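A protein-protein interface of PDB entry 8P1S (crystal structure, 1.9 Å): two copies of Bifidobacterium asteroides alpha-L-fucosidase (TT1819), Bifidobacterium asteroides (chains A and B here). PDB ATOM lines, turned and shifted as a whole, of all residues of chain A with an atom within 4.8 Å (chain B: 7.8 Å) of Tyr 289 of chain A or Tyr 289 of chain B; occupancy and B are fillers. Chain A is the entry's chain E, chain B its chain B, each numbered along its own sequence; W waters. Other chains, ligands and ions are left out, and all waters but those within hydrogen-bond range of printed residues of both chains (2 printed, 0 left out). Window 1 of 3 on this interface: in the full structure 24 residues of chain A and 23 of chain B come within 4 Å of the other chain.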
ATOM      1  N   LEU A  24     -33.981  -7.924   8.085  1.00  0.00           N
ATOM      2  CA  LEU A  24     -33.329  -9.037   7.425  1.00  0.00           C
ATOM      3  C   LEU A  24     -33.073  -8.699   5.952  1.00  0.00           C
ATOM      4  O   LEU A  24     -32.027  -9.046   5.425  1.00  0.00           O
ATOM      5  CB  LEU A  24     -34.185 -10.300   7.499  1.00  0.00           C
ATOM      6  CG  LEU A  24     -34.422 -10.905   8.888  1.00  0.00           C
ATOM      7  CD1 LEU A  24     -35.322 -12.111   8.794  1.00  0.00           C
ATOM      8  CD2 LEU A  24     -33.182 -11.411   9.488  1.00  0.00           C
ATOM      9  N   LEU A  25     -34.028  -8.103   5.260  1.00  0.00           N
ATOM     10  CA  LEU A  25     -33.847  -7.785   3.839  1.00  0.00           C
ATOM     11  C   LEU A  25     -32.834  -6.663   3.655  1.00  0.00           C
ATOM     12  O   LEU A  25     -32.087  -6.623   2.683  1.00  0.00           O
ATOM     13  CB  LEU A  25     -35.183  -7.396   3.245  1.00  0.00           C
ATOM     14  CG  LEU A  25     -36.203  -8.515   3.076  1.00  0.00           C
ATOM     15  CD1 LEU A  25     -37.488  -7.954   2.517  1.00  0.00           C
ATOM     16  CD2 LEU A  25     -35.703  -9.600   2.139  1.00  0.00           C
ATOM     17  N   GLY A  26     -32.818  -5.753   4.611  1.00  0.00           N
ATOM     18  CA  GLY A  26     -31.777  -4.746   4.709  1.00  0.00           C
ATOM     19  C   GLY A  26     -31.738  -3.827   3.483  1.00  0.00           C
ATOM     20  O   GLY A  26     -30.679  -3.421   3.074  1.00  0.00           O
ATOM     21  N   PHE A 287     -32.621  -0.913   9.323  1.00  0.00           N
ATOM     22  CA  PHE A 287     -31.308  -1.305   8.802  1.00  0.00           C
ATOM     23  C   PHE A 287     -31.313  -1.468   7.264  1.00  0.00           C
ATOM     24  O   PHE A 287     -32.154  -2.136   6.667  1.00  0.00           O
ATOM     25  CB  PHE A 287     -30.846  -2.584   9.493  1.00  0.00           C
ATOM     26  CG  PHE A 287     -29.480  -3.074   9.061  1.00  0.00           C
ATOM     27  CD1 PHE A 287     -28.330  -2.443   9.478  1.00  0.00           C
ATOM     28  CD2 PHE A 287     -29.357  -4.130   8.172  1.00  0.00           C
ATOM     29  CE1 PHE A 287     -27.086  -2.805   9.019  1.00  0.00           C
ATOM     30  CE2 PHE A 287     -28.100  -4.543   7.735  1.00  0.00           C
ATOM     31  CZ  PHE A 287     -26.962  -3.854   8.133  1.00  0.00           C
ATOM     32  N   ALA A 288     -30.333  -0.868   6.629  1.00  0.00           N
ATOM     33  CA  ALA A 288     -30.096  -0.962   5.197  1.00  0.00           C
ATOM     34  C   ALA A 288     -28.600  -1.211   4.925  1.00  0.00           C
ATOM     35  O   ALA A 288     -27.754  -0.350   5.216  1.00  0.00           O
ATOM     36  CB  ALA A 288     -30.576   0.309   4.535  1.00  0.00           C
ATOM     37  N   TYR A 289     -28.274  -2.342   4.260  1.00  0.00           N
ATOM     38  CA  TYR A 289     -26.876  -2.672   3.909  1.00  0.00           C
ATOM     39  C   TYR A 289     -26.275  -1.487   3.144  1.00  0.00           C
ATOM     40  O   TYR A 289     -25.147  -1.079   3.390  1.00  0.00           O
ATOM     41  CB  TYR A 289     -26.751  -3.960   3.064  1.00  0.00           C
ATOM     42  CG  TYR A 289     -27.115  -5.233   3.807  1.00  0.00           C
ATOM     43  CD1 TYR A 289     -26.332  -5.694   4.865  1.00  0.00           C
ATOM     44  CD2 TYR A 289     -28.203  -6.009   3.476  1.00  0.00           C
ATOM     45  CE1 TYR A 289     -26.618  -6.885   5.540  1.00  0.00           C
ATOM     46  CE2 TYR A 289     -28.556  -7.161   4.168  1.00  0.00           C
ATOM     47  CZ  TYR A 289     -27.744  -7.624   5.186  1.00  0.00           C
ATOM     48  OH  TYR A 289     -28.126  -8.734   5.876  1.00  0.00           O
ATOM     49  N   HIS A 290     -27.015  -0.964   2.179  1.00  0.00           N
ATOM     50  CA  HIS A 290     -26.516   0.011   1.221  1.00  0.00           C
ATOM     51  C   HIS A 290     -26.220   1.360   1.889  1.00  0.00           C
ATOM     52  O   HIS A 290     -25.368   2.088   1.396  1.00  0.00           O
ATOM     53  CB  HIS A 290     -27.469   0.201   0.035  1.00  0.00           C
ATOM     54  CG  HIS A 290     -28.825   0.763   0.393  1.00  0.00           C
ATOM     55  ND1 HIS A 290     -30.025   0.062   0.163  1.00  0.00           N
ATOM     56  CD2 HIS A 290     -29.169   1.969   0.913  1.00  0.00           C
ATOM     57  CE1 HIS A 290     -31.042   0.819   0.554  1.00  0.00           C
ATOM     58  NE2 HIS A 290     -30.524   1.989   0.985  1.00  0.00           N
ATOM     59  N   ASP A 291     -26.796   1.647   3.047  1.00  0.00           N
ATOM     60  CA  ASP A 291     -26.651   2.983   3.621  1.00  0.00           C
ATOM     61  C   ASP A 291     -25.471   3.064   4.600  1.00  0.00           C
ATOM     62  O   ASP A 291     -25.560   2.653   5.779  1.00  0.00           O
ATOM     63  CB  ASP A 291     -27.976   3.443   4.247  1.00  0.00           C
ATOM     64  CG  ASP A 291     -27.940   4.855   4.795  1.00  0.00           C
ATOM     65  OD1 ASP A 291     -26.877   5.524   4.697  1.00  0.00           O
ATOM     66  OD2 ASP A 291     -29.003   5.289   5.300  1.00  0.00           O
ATOM     67  N   GLN A 292     -24.379   3.646   4.108  1.00  0.00           N
ATOM     68  CA  GLN A 292     -23.191   3.911   4.927  1.00  0.00           C
ATOM     69  C   GLN A 292     -23.000   5.406   5.156  1.00  0.00           C
ATOM     70  O   GLN A 292     -21.912   5.839   5.485  1.00  0.00           O
ATOM     71  CB  GLN A 292     -21.958   3.355   4.217  1.00  0.00           C
ATOM     72  CG  GLN A 292     -22.060   1.855   4.026  1.00  0.00           C
ATOM     73  CD  GLN A 292     -22.226   1.088   5.304  1.00  0.00           C
ATOM     74  OE1 GLN A 292     -21.634   1.379   6.324  1.00  0.00           O
ATOM     75  NE2 GLN A 292     -23.087   0.102   5.257  1.00  0.00           N
ATOM     76  N   ASP A 321     -29.654  -4.701  12.985  1.00  0.00           N
ATOM     77  CA  ASP A 321     -29.499  -5.623  11.865  1.00  0.00           C
ATOM     78  C   ASP A 321     -30.230  -6.943  12.149  1.00  0.00           C
ATOM     79  O   ASP A 321     -30.902  -7.107  13.149  1.00  0.00           O
ATOM     80  CB  ASP A 321     -27.999  -5.807  11.487  1.00  0.00           C
ATOM     81  CG  ASP A 321     -27.226  -6.679  12.481  1.00  0.00           C
ATOM     82  OD1 ASP A 321     -27.907  -7.350  13.373  1.00  0.00           O
ATOM     83  OD2 ASP A 321     -25.960  -6.645  12.407  1.00  0.00           O
ATOM     84  N   LEU A 323     -29.286  -9.790  12.908  1.00  0.00           N
ATOM     85  CA  LEU A 323     -28.827 -10.576  14.044  1.00  0.00           C
ATOM     86  C   LEU A 323     -29.116  -9.914  15.394  1.00  0.00           C
ATOM     87  O   LEU A 323     -28.764 -10.467  16.454  1.00  0.00           O
ATOM     88  CB  LEU A 323     -27.322 -10.781  13.902  1.00  0.00           C
ATOM     89  CG  LEU A 323     -26.911 -11.783  12.814  1.00  0.00           C
ATOM     90  CD1 LEU A 323     -25.402 -11.755  12.583  1.00  0.00           C
ATOM     91  CD2 LEU A 323     -27.423 -13.181  13.196  1.00  0.00           C
ATOM     92  N   ARG A 325     -28.248  -6.662  16.222  1.00  0.00           N
ATOM     93  CA  ARG A 325     -27.125  -5.901  16.671  1.00  0.00           C
ATOM     94  C   ARG A 325     -27.307  -4.424  16.276  1.00  0.00           C
ATOM     95  O   ARG A 325     -27.818  -4.082  15.201  1.00  0.00           O
ATOM     96  CB  ARG A 325     -25.819  -6.346  15.997  1.00  0.00           C
ATOM     97  CG  ARG A 325     -25.511  -7.831  16.141  1.00  0.00           C
ATOM     98  CD  ARG A 325     -24.211  -8.291  15.562  1.00  0.00           C
ATOM     99  NE  ARG A 325     -24.255  -8.185  14.106  1.00  0.00           N
ATOM    100  CZ  ARG A 325     -23.234  -8.501  13.301  1.00  0.00           C
ATOM    101  NH1 ARG A 325     -22.139  -9.031  13.814  1.00  0.00           N
ATOM    102  NH2 ARG A 325     -23.283  -8.240  12.004  1.00  0.00           N
ATOM    103  N   TYR B  22     -19.093 -16.892   8.354  1.00  0.00           N
ATOM    104  CA  TYR B  22     -18.551 -15.519   8.350  1.00  0.00           C
ATOM    105  C   TYR B  22     -19.465 -14.507   7.628  1.00  0.00           C
ATOM    106  O   TYR B  22     -19.453 -13.328   7.967  1.00  0.00           O
ATOM    107  CB  TYR B  22     -17.147 -15.481   7.730  1.00  0.00           C
ATOM    108  CG  TYR B  22     -16.935 -16.168   6.418  1.00  0.00           C
ATOM    109  CD1 TYR B  22     -17.295 -15.565   5.223  1.00  0.00           C
ATOM    110  CD2 TYR B  22     -16.379 -17.456   6.365  1.00  0.00           C
ATOM    111  CE1 TYR B  22     -17.193 -16.257   4.016  1.00  0.00           C
ATOM    112  CE2 TYR B  22     -16.269 -18.148   5.168  1.00  0.00           C
ATOM    113  CZ  TYR B  22     -16.656 -17.530   3.985  1.00  0.00           C
ATOM    114  OH  TYR B  22     -16.516 -18.253   2.839  1.00  0.00           O
ATOM    115  N   SER B  23     -20.213 -14.967   6.631  1.00  0.00           N
ATOM    116  CA  SER B  23     -21.090 -14.109   5.839  1.00  0.00           C
ATOM    117  C   SER B  23     -22.220 -13.526   6.698  1.00  0.00           C
ATOM    118  O   SER B  23     -22.777 -12.470   6.388  1.00  0.00           O
ATOM    119  CB  SER B  23     -21.699 -14.956   4.713  1.00  0.00           C
ATOM    120  OG  SER B  23     -20.691 -15.627   3.938  1.00  0.00           O
ATOM    121  N   LEU B  24     -22.641 -14.252   7.763  1.00  0.00           N
ATOM    122  CA  LEU B  24     -23.658 -13.742   8.659  1.00  0.00           C
ATOM    123  C   LEU B  24     -23.105 -12.571   9.434  1.00  0.00           C
ATOM    124  O   LEU B  24     -23.832 -11.618   9.694  1.00  0.00           O
ATOM    125  CB  LEU B  24     -24.132 -14.847   9.619  1.00  0.00           C
ATOM    126  CG  LEU B  24     -24.836 -16.064   9.020  1.00  0.00           C
ATOM    127  CD1 LEU B  24     -25.061 -17.147  10.085  1.00  0.00           C
ATOM    128  CD2 LEU B  24     -26.137 -15.677   8.460  1.00  0.00           C
ATOM    129  N   LEU B  25     -21.863 -12.675   9.952  1.00  0.00           N
ATOM    130  CA  LEU B  25     -21.311 -11.590  10.745  1.00  0.00           C
ATOM    131  C   LEU B  25     -21.024 -10.358   9.872  1.00  0.00           C
ATOM    132  O   LEU B  25     -21.134  -9.186  10.322  1.00  0.00           O
ATOM    133  CB  LEU B  25     -20.044 -12.067  11.394  1.00  0.00           C
ATOM    134  CG  LEU B  25     -20.222 -13.063  12.554  1.00  0.00           C
ATOM    135  CD1 LEU B  25     -18.829 -13.486  13.038  1.00  0.00           C
ATOM    136  CD2 LEU B  25     -21.031 -12.507  13.699  1.00  0.00           C
ATOM    137  N   GLY B  26     -20.675 -10.621   8.627  1.00  0.00           N
ATOM    138  CA  GLY B  26     -20.612  -9.523   7.666  1.00  0.00           C
ATOM    139  C   GLY B  26     -19.541  -8.494   7.993  1.00  0.00           C
ATOM    140  O   GLY B  26     -19.703  -7.335   7.687  1.00  0.00           O
ATOM    141  N   GLY B  27     -18.479  -8.896   8.686  1.00  0.00           N
ATOM    142  CA  GLY B  27     -17.368  -8.014   8.923  1.00  0.00           C
ATOM    143  C   GLY B  27     -17.363  -7.350  10.289  1.00  0.00           C
ATOM    144  O   GLY B  27     -16.555  -6.462  10.547  1.00  0.00           O
ATOM    145  N   GLU B  28     -18.308  -7.719  11.158  1.00  0.00           N
ATOM    146  CA  GLU B  28     -18.347  -7.144  12.503  1.00  0.00           C
ATOM    147  C   GLU B  28     -18.762  -8.185  13.529  1.00  0.00           C
ATOM    148  O   GLU B  28     -19.385  -9.190  13.172  1.00  0.00           O
ATOM    149  CB  GLU B  28     -19.136  -5.839  12.669  1.00  0.00           C
ATOM    150  CG  GLU B  28     -20.286  -5.578  11.785  1.00  0.00           C
ATOM    151  CD  GLU B  28     -20.876  -4.187  11.882  1.00  0.00           C
ATOM    152  OE1 GLU B  28     -21.484  -3.869  12.906  1.00  0.00           O
ATOM    153  OE2 GLU B  28     -20.682  -3.446  10.954  1.00  0.00           O
ATOM    154  N   ALA B  38     -13.745  -9.891   5.515  1.00  0.00           N
ATOM    155  CA  ALA B  38     -14.786 -10.323   6.443  1.00  0.00           C
ATOM    156  C   ALA B  38     -14.712 -11.809   6.768  1.00  0.00           C
ATOM    157  O   ALA B  38     -15.095 -12.261   7.879  1.00  0.00           O
ATOM    158  CB  ALA B  38     -16.124  -9.969   5.882  1.00  0.00           C
ATOM    159  N   ASN B 282     -16.421  -5.629  -4.883  1.00  0.00           N
ATOM    160  CA  ASN B 282     -16.003  -4.600  -3.939  1.00  0.00           C
ATOM    161  C   ASN B 282     -14.582  -4.981  -3.513  1.00  0.00           C
ATOM    162  O   ASN B 282     -13.814  -5.511  -4.340  1.00  0.00           O
ATOM    163  CB  ASN B 282     -17.072  -4.369  -2.875  1.00  0.00           C
ATOM    164  CG  ASN B 282     -17.399  -5.613  -2.051  1.00  0.00           C
ATOM    165  OD1 ASN B 282     -16.820  -6.686  -2.222  1.00  0.00           O
ATOM    166  ND2 ASN B 282     -18.343  -5.469  -1.124  1.00  0.00           N
ATOM    167  N   SER B 284     -13.971  -7.092  -0.687  1.00  0.00           N
ATOM    168  CA  SER B 284     -14.021  -8.187   0.282  1.00  0.00           C
ATOM    169  C   SER B 284     -14.378  -9.445  -0.500  1.00  0.00           C
ATOM    170  O   SER B 284     -14.991  -9.433  -1.598  1.00  0.00           O
ATOM    171  CB  SER B 284     -14.942  -7.946   1.559  1.00  0.00           C
ATOM    172  OG  SER B 284     -14.802  -9.029   2.713  1.00  0.00           O
ATOM    173  N   GLY B 286     -15.527 -12.495   1.434  1.00  0.00           N
ATOM    174  CA  GLY B 286     -16.762 -12.707   2.153  1.00  0.00           C
ATOM    175  C   GLY B 286     -17.616 -11.432   2.176  1.00  0.00           C
ATOM    176  O   GLY B 286     -17.125 -10.317   2.093  1.00  0.00           O
ATOM    177  N   PHE B 287     -18.917 -11.612   2.242  1.00  0.00           N
ATOM    178  CA  PHE B 287     -19.841 -10.483   2.372  1.00  0.00           C
ATOM    179  C   PHE B 287     -19.479  -9.635   3.599  1.00  0.00           C
ATOM    180  O   PHE B 287     -19.281 -10.133   4.717  1.00  0.00           O
ATOM    181  CB  PHE B 287     -21.280 -11.012   2.490  1.00  0.00           C
ATOM    182  CG  PHE B 287     -22.335  -9.963   2.656  1.00  0.00           C
ATOM    183  CD1 PHE B 287     -22.718  -9.166   1.573  1.00  0.00           C
ATOM    184  CD2 PHE B 287     -22.882  -9.725   3.889  1.00  0.00           C
ATOM    185  CE1 PHE B 287     -23.727  -8.210   1.708  1.00  0.00           C
ATOM    186  CE2 PHE B 287     -23.869  -8.747   4.027  1.00  0.00           C
ATOM    187  CZ  PHE B 287     -24.273  -7.976   2.937  1.00  0.00           C
ATOM    188  N   ALA B 288     -19.384  -8.319   3.372  1.00  0.00           N
ATOM    189  CA  ALA B 288     -19.115  -7.356   4.428  1.00  0.00           C
ATOM    190  C   ALA B 288     -20.149  -6.211   4.346  1.00  0.00           C
ATOM    191  O   ALA B 288     -20.211  -5.505   3.333  1.00  0.00           O
ATOM    192  CB  ALA B 288     -17.727  -6.835   4.259  1.00  0.00           C
ATOM    193  N   TYR B 289     -20.934  -6.008   5.437  1.00  0.00           N
ATOM    194  CA  TYR B 289     -22.027  -5.017   5.457  1.00  0.00           C
ATOM    195  C   TYR B 289     -21.498  -3.675   4.971  1.00  0.00           C
ATOM    196  O   TYR B 289     -22.101  -3.026   4.092  1.00  0.00           O
ATOM    197  CB  TYR B 289     -22.675  -4.870   6.845  1.00  0.00           C
ATOM    198  CG  TYR B 289     -23.377  -6.090   7.454  1.00  0.00           C
ATOM    199  CD1 TYR B 289     -23.326  -7.379   6.982  1.00  0.00           C
ATOM    200  CD2 TYR B 289     -24.108  -5.939   8.612  1.00  0.00           C
ATOM    201  CE1 TYR B 289     -24.042  -8.448   7.544  1.00  0.00           C
ATOM    202  CE2 TYR B 289     -24.851  -6.974   9.180  1.00  0.00           C
ATOM    203  CZ  TYR B 289     -24.845  -8.233   8.627  1.00  0.00           C
ATOM    204  OH  TYR B 289     -25.553  -9.230   9.225  1.00  0.00           O
ATOM    205  N   HIS B 290     -20.353  -3.277   5.563  1.00  0.00           N
ATOM    206  CA  HIS B 290     -19.800  -1.955   5.469  1.00  0.00           C
ATOM    207  C   HIS B 290     -19.323  -1.677   4.038  1.00  0.00           C
ATOM    208  O   HIS B 290     -19.295  -0.523   3.640  1.00  0.00           O
ATOM    209  CB  HIS B 290     -18.652  -1.779   6.488  1.00  0.00           C
ATOM    210  CG  HIS B 290     -17.363  -2.482   6.144  1.00  0.00           C
ATOM    211  ND1 HIS B 290     -16.803  -3.700   6.543  1.00  0.00           N
ATOM    212  CD2 HIS B 290     -16.513  -1.929   5.195  1.00  0.00           C
ATOM    213  CE1 HIS B 290     -15.660  -3.861   5.892  1.00  0.00           C
ATOM    214  NE2 HIS B 290     -15.442  -2.791   5.071  1.00  0.00           N
ATOM    215  N   ASP B 291     -18.953  -2.701   3.251  1.00  0.00           N
ATOM    216  CA  ASP B 291     -18.167  -2.451   2.048  1.00  0.00           C
ATOM    217  C   ASP B 291     -19.113  -2.231   0.850  1.00  0.00           C
ATOM    218  O   ASP B 291     -19.711  -3.176   0.287  1.00  0.00           O
ATOM    219  CB  ASP B 291     -17.182  -3.604   1.781  1.00  0.00           C
ATOM    220  CG  ASP B 291     -16.359  -3.448   0.504  1.00  0.00           C
ATOM    221  OD1 ASP B 291     -16.503  -2.389  -0.185  1.00  0.00           O
ATOM    222  OD2 ASP B 291     -15.571  -4.358   0.199  1.00  0.00           O
ATOM    223  N   GLN B 292     -19.263  -0.961   0.492  1.00  0.00           N
ATOM    224  CA  GLN B 292     -20.051  -0.541  -0.655  1.00  0.00           C
ATOM    225  C   GLN B 292     -19.136   0.036  -1.724  1.00  0.00           C
ATOM    226  O   GLN B 292     -19.593   0.781  -2.576  1.00  0.00           O
ATOM    227  CB  GLN B 292     -21.077   0.517  -0.226  1.00  0.00           C
ATOM    228  CG  GLN B 292     -21.984   0.041   0.887  1.00  0.00           C
ATOM    229  CD  GLN B 292     -22.794  -1.146   0.452  1.00  0.00           C
ATOM    230  OE1 GLN B 292     -23.277  -1.096  -0.668  1.00  0.00           O
ATOM    231  NE2 GLN B 292     -22.927  -2.203   1.239  1.00  0.00           N
ATOM    232  N   ASN B 293     -17.850  -0.306  -1.732  1.00  0.00           N
ATOM    233  CA  ASN B 293     -16.955   0.228  -2.756  1.00  0.00           C
ATOM    234  C   ASN B 293     -16.960  -0.669  -4.014  1.00  0.00           C
ATOM    235  O   ASN B 293     -15.965  -1.287  -4.382  1.00  0.00           O
ATOM    236  CB  ASN B 293     -15.568   0.356  -2.143  1.00  0.00           C
ATOM    237  CG  ASN B 293     -14.646   1.123  -3.052  1.00  0.00           C
ATOM    238  OD1 ASN B 293     -15.083   2.017  -3.778  1.00  0.00           O
ATOM    239  ND2 ASN B 293     -13.387   0.721  -3.067  1.00  0.00           N
ATOM    240  N   TRP B 294     -18.125  -0.777  -4.667  1.00  0.00           N
ATOM    241  CA  TRP B 294     -18.370  -1.687  -5.772  1.00  0.00           C
ATOM    242  C   TRP B 294     -17.729  -1.118  -7.034  1.00  0.00           C
ATOM    243  O   TRP B 294     -18.014  -0.007  -7.394  1.00  0.00           O
ATOM    244  CB  TRP B 294     -19.884  -1.846  -5.988  1.00  0.00           C
ATOM    245  CG  TRP B 294     -20.599  -2.427  -4.812  1.00  0.00           C
ATOM    246  CD1 TRP B 294     -21.392  -1.718  -3.961  1.00  0.00           C
ATOM    247  CD2 TRP B 294     -20.643  -3.792  -4.359  1.00  0.00           C
ATOM    248  NE1 TRP B 294     -21.886  -2.560  -2.989  1.00  0.00           N
ATOM    249  CE2 TRP B 294     -21.433  -3.820  -3.194  1.00  0.00           C
ATOM    250  CE3 TRP B 294     -20.086  -4.988  -4.797  1.00  0.00           C
ATOM    251  CZ2 TRP B 294     -21.703  -4.987  -2.478  1.00  0.00           C
ATOM    252  CZ3 TRP B 294     -20.350  -6.150  -4.104  1.00  0.00           C
ATOM    253  CH2 TRP B 294     -21.149  -6.149  -2.958  1.00  0.00           C
ATOM    254  N   ASP B 321     -24.673 -13.078   0.778  1.00  0.00           N
ATOM    255  CA  ASP B 321     -25.056 -12.567   2.085  1.00  0.00           C
ATOM    256  C   ASP B 321     -25.632 -13.716   2.941  1.00  0.00           C
ATOM    257  O   ASP B 321     -25.654 -14.879   2.524  1.00  0.00           O
ATOM    258  CB  ASP B 321     -25.971 -11.347   1.994  1.00  0.00           C
ATOM    259  CG  ASP B 321     -27.366 -11.636   1.540  1.00  0.00           C
ATOM    260  OD1 ASP B 321     -27.737 -12.839   1.524  1.00  0.00           O
ATOM    261  OD2 ASP B 321     -28.092 -10.632   1.241  1.00  0.00           O
ATOM    262  N   GLY B 322     -26.044 -13.359   4.152  1.00  0.00           N
ATOM    263  CA  GLY B 322     -26.531 -14.311   5.157  1.00  0.00           C
ATOM    264  C   GLY B 322     -27.821 -14.988   4.737  1.00  0.00           C
ATOM    265  O   GLY B 322     -28.195 -16.006   5.294  1.00  0.00           O
ATOM    266  N   LEU B 323     -28.527 -14.407   3.745  1.00  0.00           N
ATOM    267  CA  LEU B 323     -29.747 -15.009   3.240  1.00  0.00           C
ATOM    268  C   LEU B 323     -29.514 -15.807   1.948  1.00  0.00           C
ATOM    269  O   LEU B 323     -30.458 -16.362   1.399  1.00  0.00           O
ATOM    270  CB  LEU B 323     -30.758 -13.903   3.007  1.00  0.00           C
ATOM    271  CG  LEU B 323     -31.333 -13.246   4.257  1.00  0.00           C
ATOM    272  CD1 LEU B 323     -32.137 -12.039   3.852  1.00  0.00           C
ATOM    273  CD2 LEU B 323     -32.157 -14.219   5.081  1.00  0.00           C
ATOM    274  N   ARG B 325     -27.974 -14.575  -0.837  1.00  0.00           N
ATOM    275  CA  ARG B 325     -28.195 -13.723  -1.999  1.00  0.00           C
ATOM    276  C   ARG B 325     -26.901 -13.202  -2.560  1.00  0.00           C
ATOM    277  O   ARG B 325     -25.998 -12.828  -1.833  1.00  0.00           O
ATOM    278  CB  ARG B 325     -29.097 -12.513  -1.676  1.00  0.00           C
ATOM    279  CG  ARG B 325     -30.413 -12.856  -1.019  1.00  0.00           C
ATOM    280  CD  ARG B 325     -31.322 -11.675  -0.803  1.00  0.00           C
ATOM    281  NE  ARG B 325     -30.746 -10.844   0.260  1.00  0.00           N
ATOM    282  CZ  ARG B 325     -31.314  -9.711   0.692  1.00  0.00           C
ATOM    283  NH1 ARG B 325     -32.526  -9.426   0.296  1.00  0.00           N
ATOM    284  NH2 ARG B 325     -30.702  -8.857   1.493  1.00  0.00           N
ATOM    285  N   PRO B 327     -25.511  -9.902  -3.564  1.00  0.00           N
ATOM    286  CA  PRO B 327     -25.868  -8.542  -3.285  1.00  0.00           C
ATOM    287  C   PRO B 327     -26.336  -7.890  -4.567  1.00  0.00           C
ATOM    288  O   PRO B 327     -25.757  -8.094  -5.593  1.00  0.00           O
ATOM    289  CB  PRO B 327     -24.604  -7.923  -2.715  1.00  0.00           C
ATOM    290  CG  PRO B 327     -23.946  -9.114  -2.061  1.00  0.00           C
ATOM    291  CD  PRO B 327     -24.157 -10.246  -3.069  1.00  0.00           C
HETATM  292  O   HOH W   1     -24.506  -4.566  11.940  1.00  0.00           O
HETATM  293  O   HOH W   2     -24.222   1.337  -1.604  1.00  0.00           O
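NH2 of Arg 325 of chain B lies within hydrogen-bond range of O of Leu 25 of chain A, at 2.9 Å. The side-chain amide nitrogen of Gln 292 of chain A lies within hydrogen-bond range of the backbone carbonyl oxygen of Tyr 289 of chain B (3.5 Å). NH1 of Arg 325 of chain A is in hydrogen-bond range of O of Glu 28 of chain B (2.8 Å). The backbone carbonyl oxygen of Leu 25 of chain B sits at hydrogen-bond distance from the guanidinium group of Arg 325 of chain A, 2.9 Å away. The side-chain amide nitrogen (NE2) of Gln 292 of chain B is in hydrogen-bond range of the backbone carbonyl oxygen (O) of Tyr 289 of chain A (3.3 Å).
The side-chain amide nitrogen (NE2) of Gln 292 of chain B lies within hydrogen-bond range of the backbone carbonyl oxygen (O) of Tyr 289 of chain B (3.1 Å). The backbone NH of Leu 323 of chain A is in hydrogen-bond range of the side-chain carboxylate of Asp 321 of chain A (2.8 Å). O of Tyr 289 of chain A lies within hydrogen-bond range of NE2 of Gln 292 of chain A (3.0 Å). O of Gly 26 of chain B is in hydrogen-bond range of N of Tyr 289 of chain B (2.9 Å). The indole nitrogen of Trp 294 of chain B lies within hydrogen-bond range of the side-chain amide oxygen of Gln 292 of chain B, 3.1 Å away.
Among the printed residues, pairs that only touch across the chains: Leu 323 of chain A with Leu 24 of chain B (3.3 Å), Leu 24 of chain A with Leu 323 of chain B (3.4 Å), Asp 321 of chain A with Tyr 289 of chain B (3.4 Å), Arg 325 of chain A with Tyr 289 of chain B (3.5 Å), Phe 287 of chain A with Tyr 289 of chain B (3.6 Å), Tyr 289 of chain A with Tyr 289 of chain B (3.6 Å), Gln 292 of chain A with Gln 292 of chain B (3.6 Å), Tyr 289 of chain A with Phe 287 of chain B (3.6 Å), Gln 292 of chain A with His 290 of chain B (3.7 Å), Tyr 289 of chain A with Arg 325 of chain B (3.8 Å) and His 290 of chain A with Gln 292 of chain B (3.9 Å).
Of chain B, only Phe 287, Tyr 289, Gln 292 and Arg 325 come within 4 Å of Tyr 289 of chain A. Of chain A, only Phe 287, Tyr 289, Gln 292, Asp 321 and Arg 325 come within 4 Å of Tyr 289 of chain B. No residue of chain B comes within 4 Å of Ala 288 of chain A. Printed residues of chain A within 4 Å of Leu 323 of chain B: Leu 24. Printed residues of chain A within 4 Å of Leu 25 of chain B: Arg 325. Of the printed residues of chain A, Phe 287 of chain B touches Tyr 289. Printed residues of chain B within 4 Å of His 290 of chain A: Gln 292 (3.9 Å). Printed residues of chain A within 4 Å of His 290 of chain B: Gln 292 (3.7 Å). The nearest residue of chain B that does not touch Tyr 289 of chain A is Asp 321 of chain B (4.6 Å). The nearest residue of chain A that does not touch Tyr 289 of chain B is Leu 323 of chain A (4.2 Å).
Of the 24 printed residues of chain B, 9 touch a printed residue of chain A. Printed residues of chain B that touch a printed residue of chain A: Leu 24, Leu 25, Glu 28, Phe 287, Tyr 289, His 290, Gln 292, Leu 323 and Arg 325. Hydrophobic or aromatic side chains of chain B within 4 Å of the printed part of chain A: Leu 25, Phe 287, Tyr 289 and Leu 323. Of the 12 printed residues of chain A, 9 touch a printed residue of chain B. Hydrophobic or aromatic side chains of chain A within 4 Å of the printed part of chain B: Leu 25, Phe 287, Tyr 289 and Leu 323. Among the printed residues, no Asp or Glu carboxylate lies within 4 Å of a Lys or Arg side-chain nitrogen of the other chain.
Leu 24 of chain A touches Leu 323 of chain B, and with the chains exchanged Leu 323 of chain A touches Leu 24 of chain B. Tyr 289 of chain A touches Gln 292 of chain B, and with the chains exchanged Gln 292 of chain A touches Tyr 289 of chain B. Tyr 289 of chain A touches Arg 325 of chain B, and with the chains exchanged Arg 325 of chain A touches Tyr 289 of chain B. His 290 of chain A touches Gln 292 of chain B, and with the chains exchanged Gln 292 of chain A touches His 290 of chain B.
Water W1 lies within hydrogen-bond range of OD2 of Asp 321 of chain A and OE1 of Glu 28 of chain B. Water W2 bridges OE1 of Gln 292 of chain B (2.8 Å) and O of His 290 of chain A (3.3 Å).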
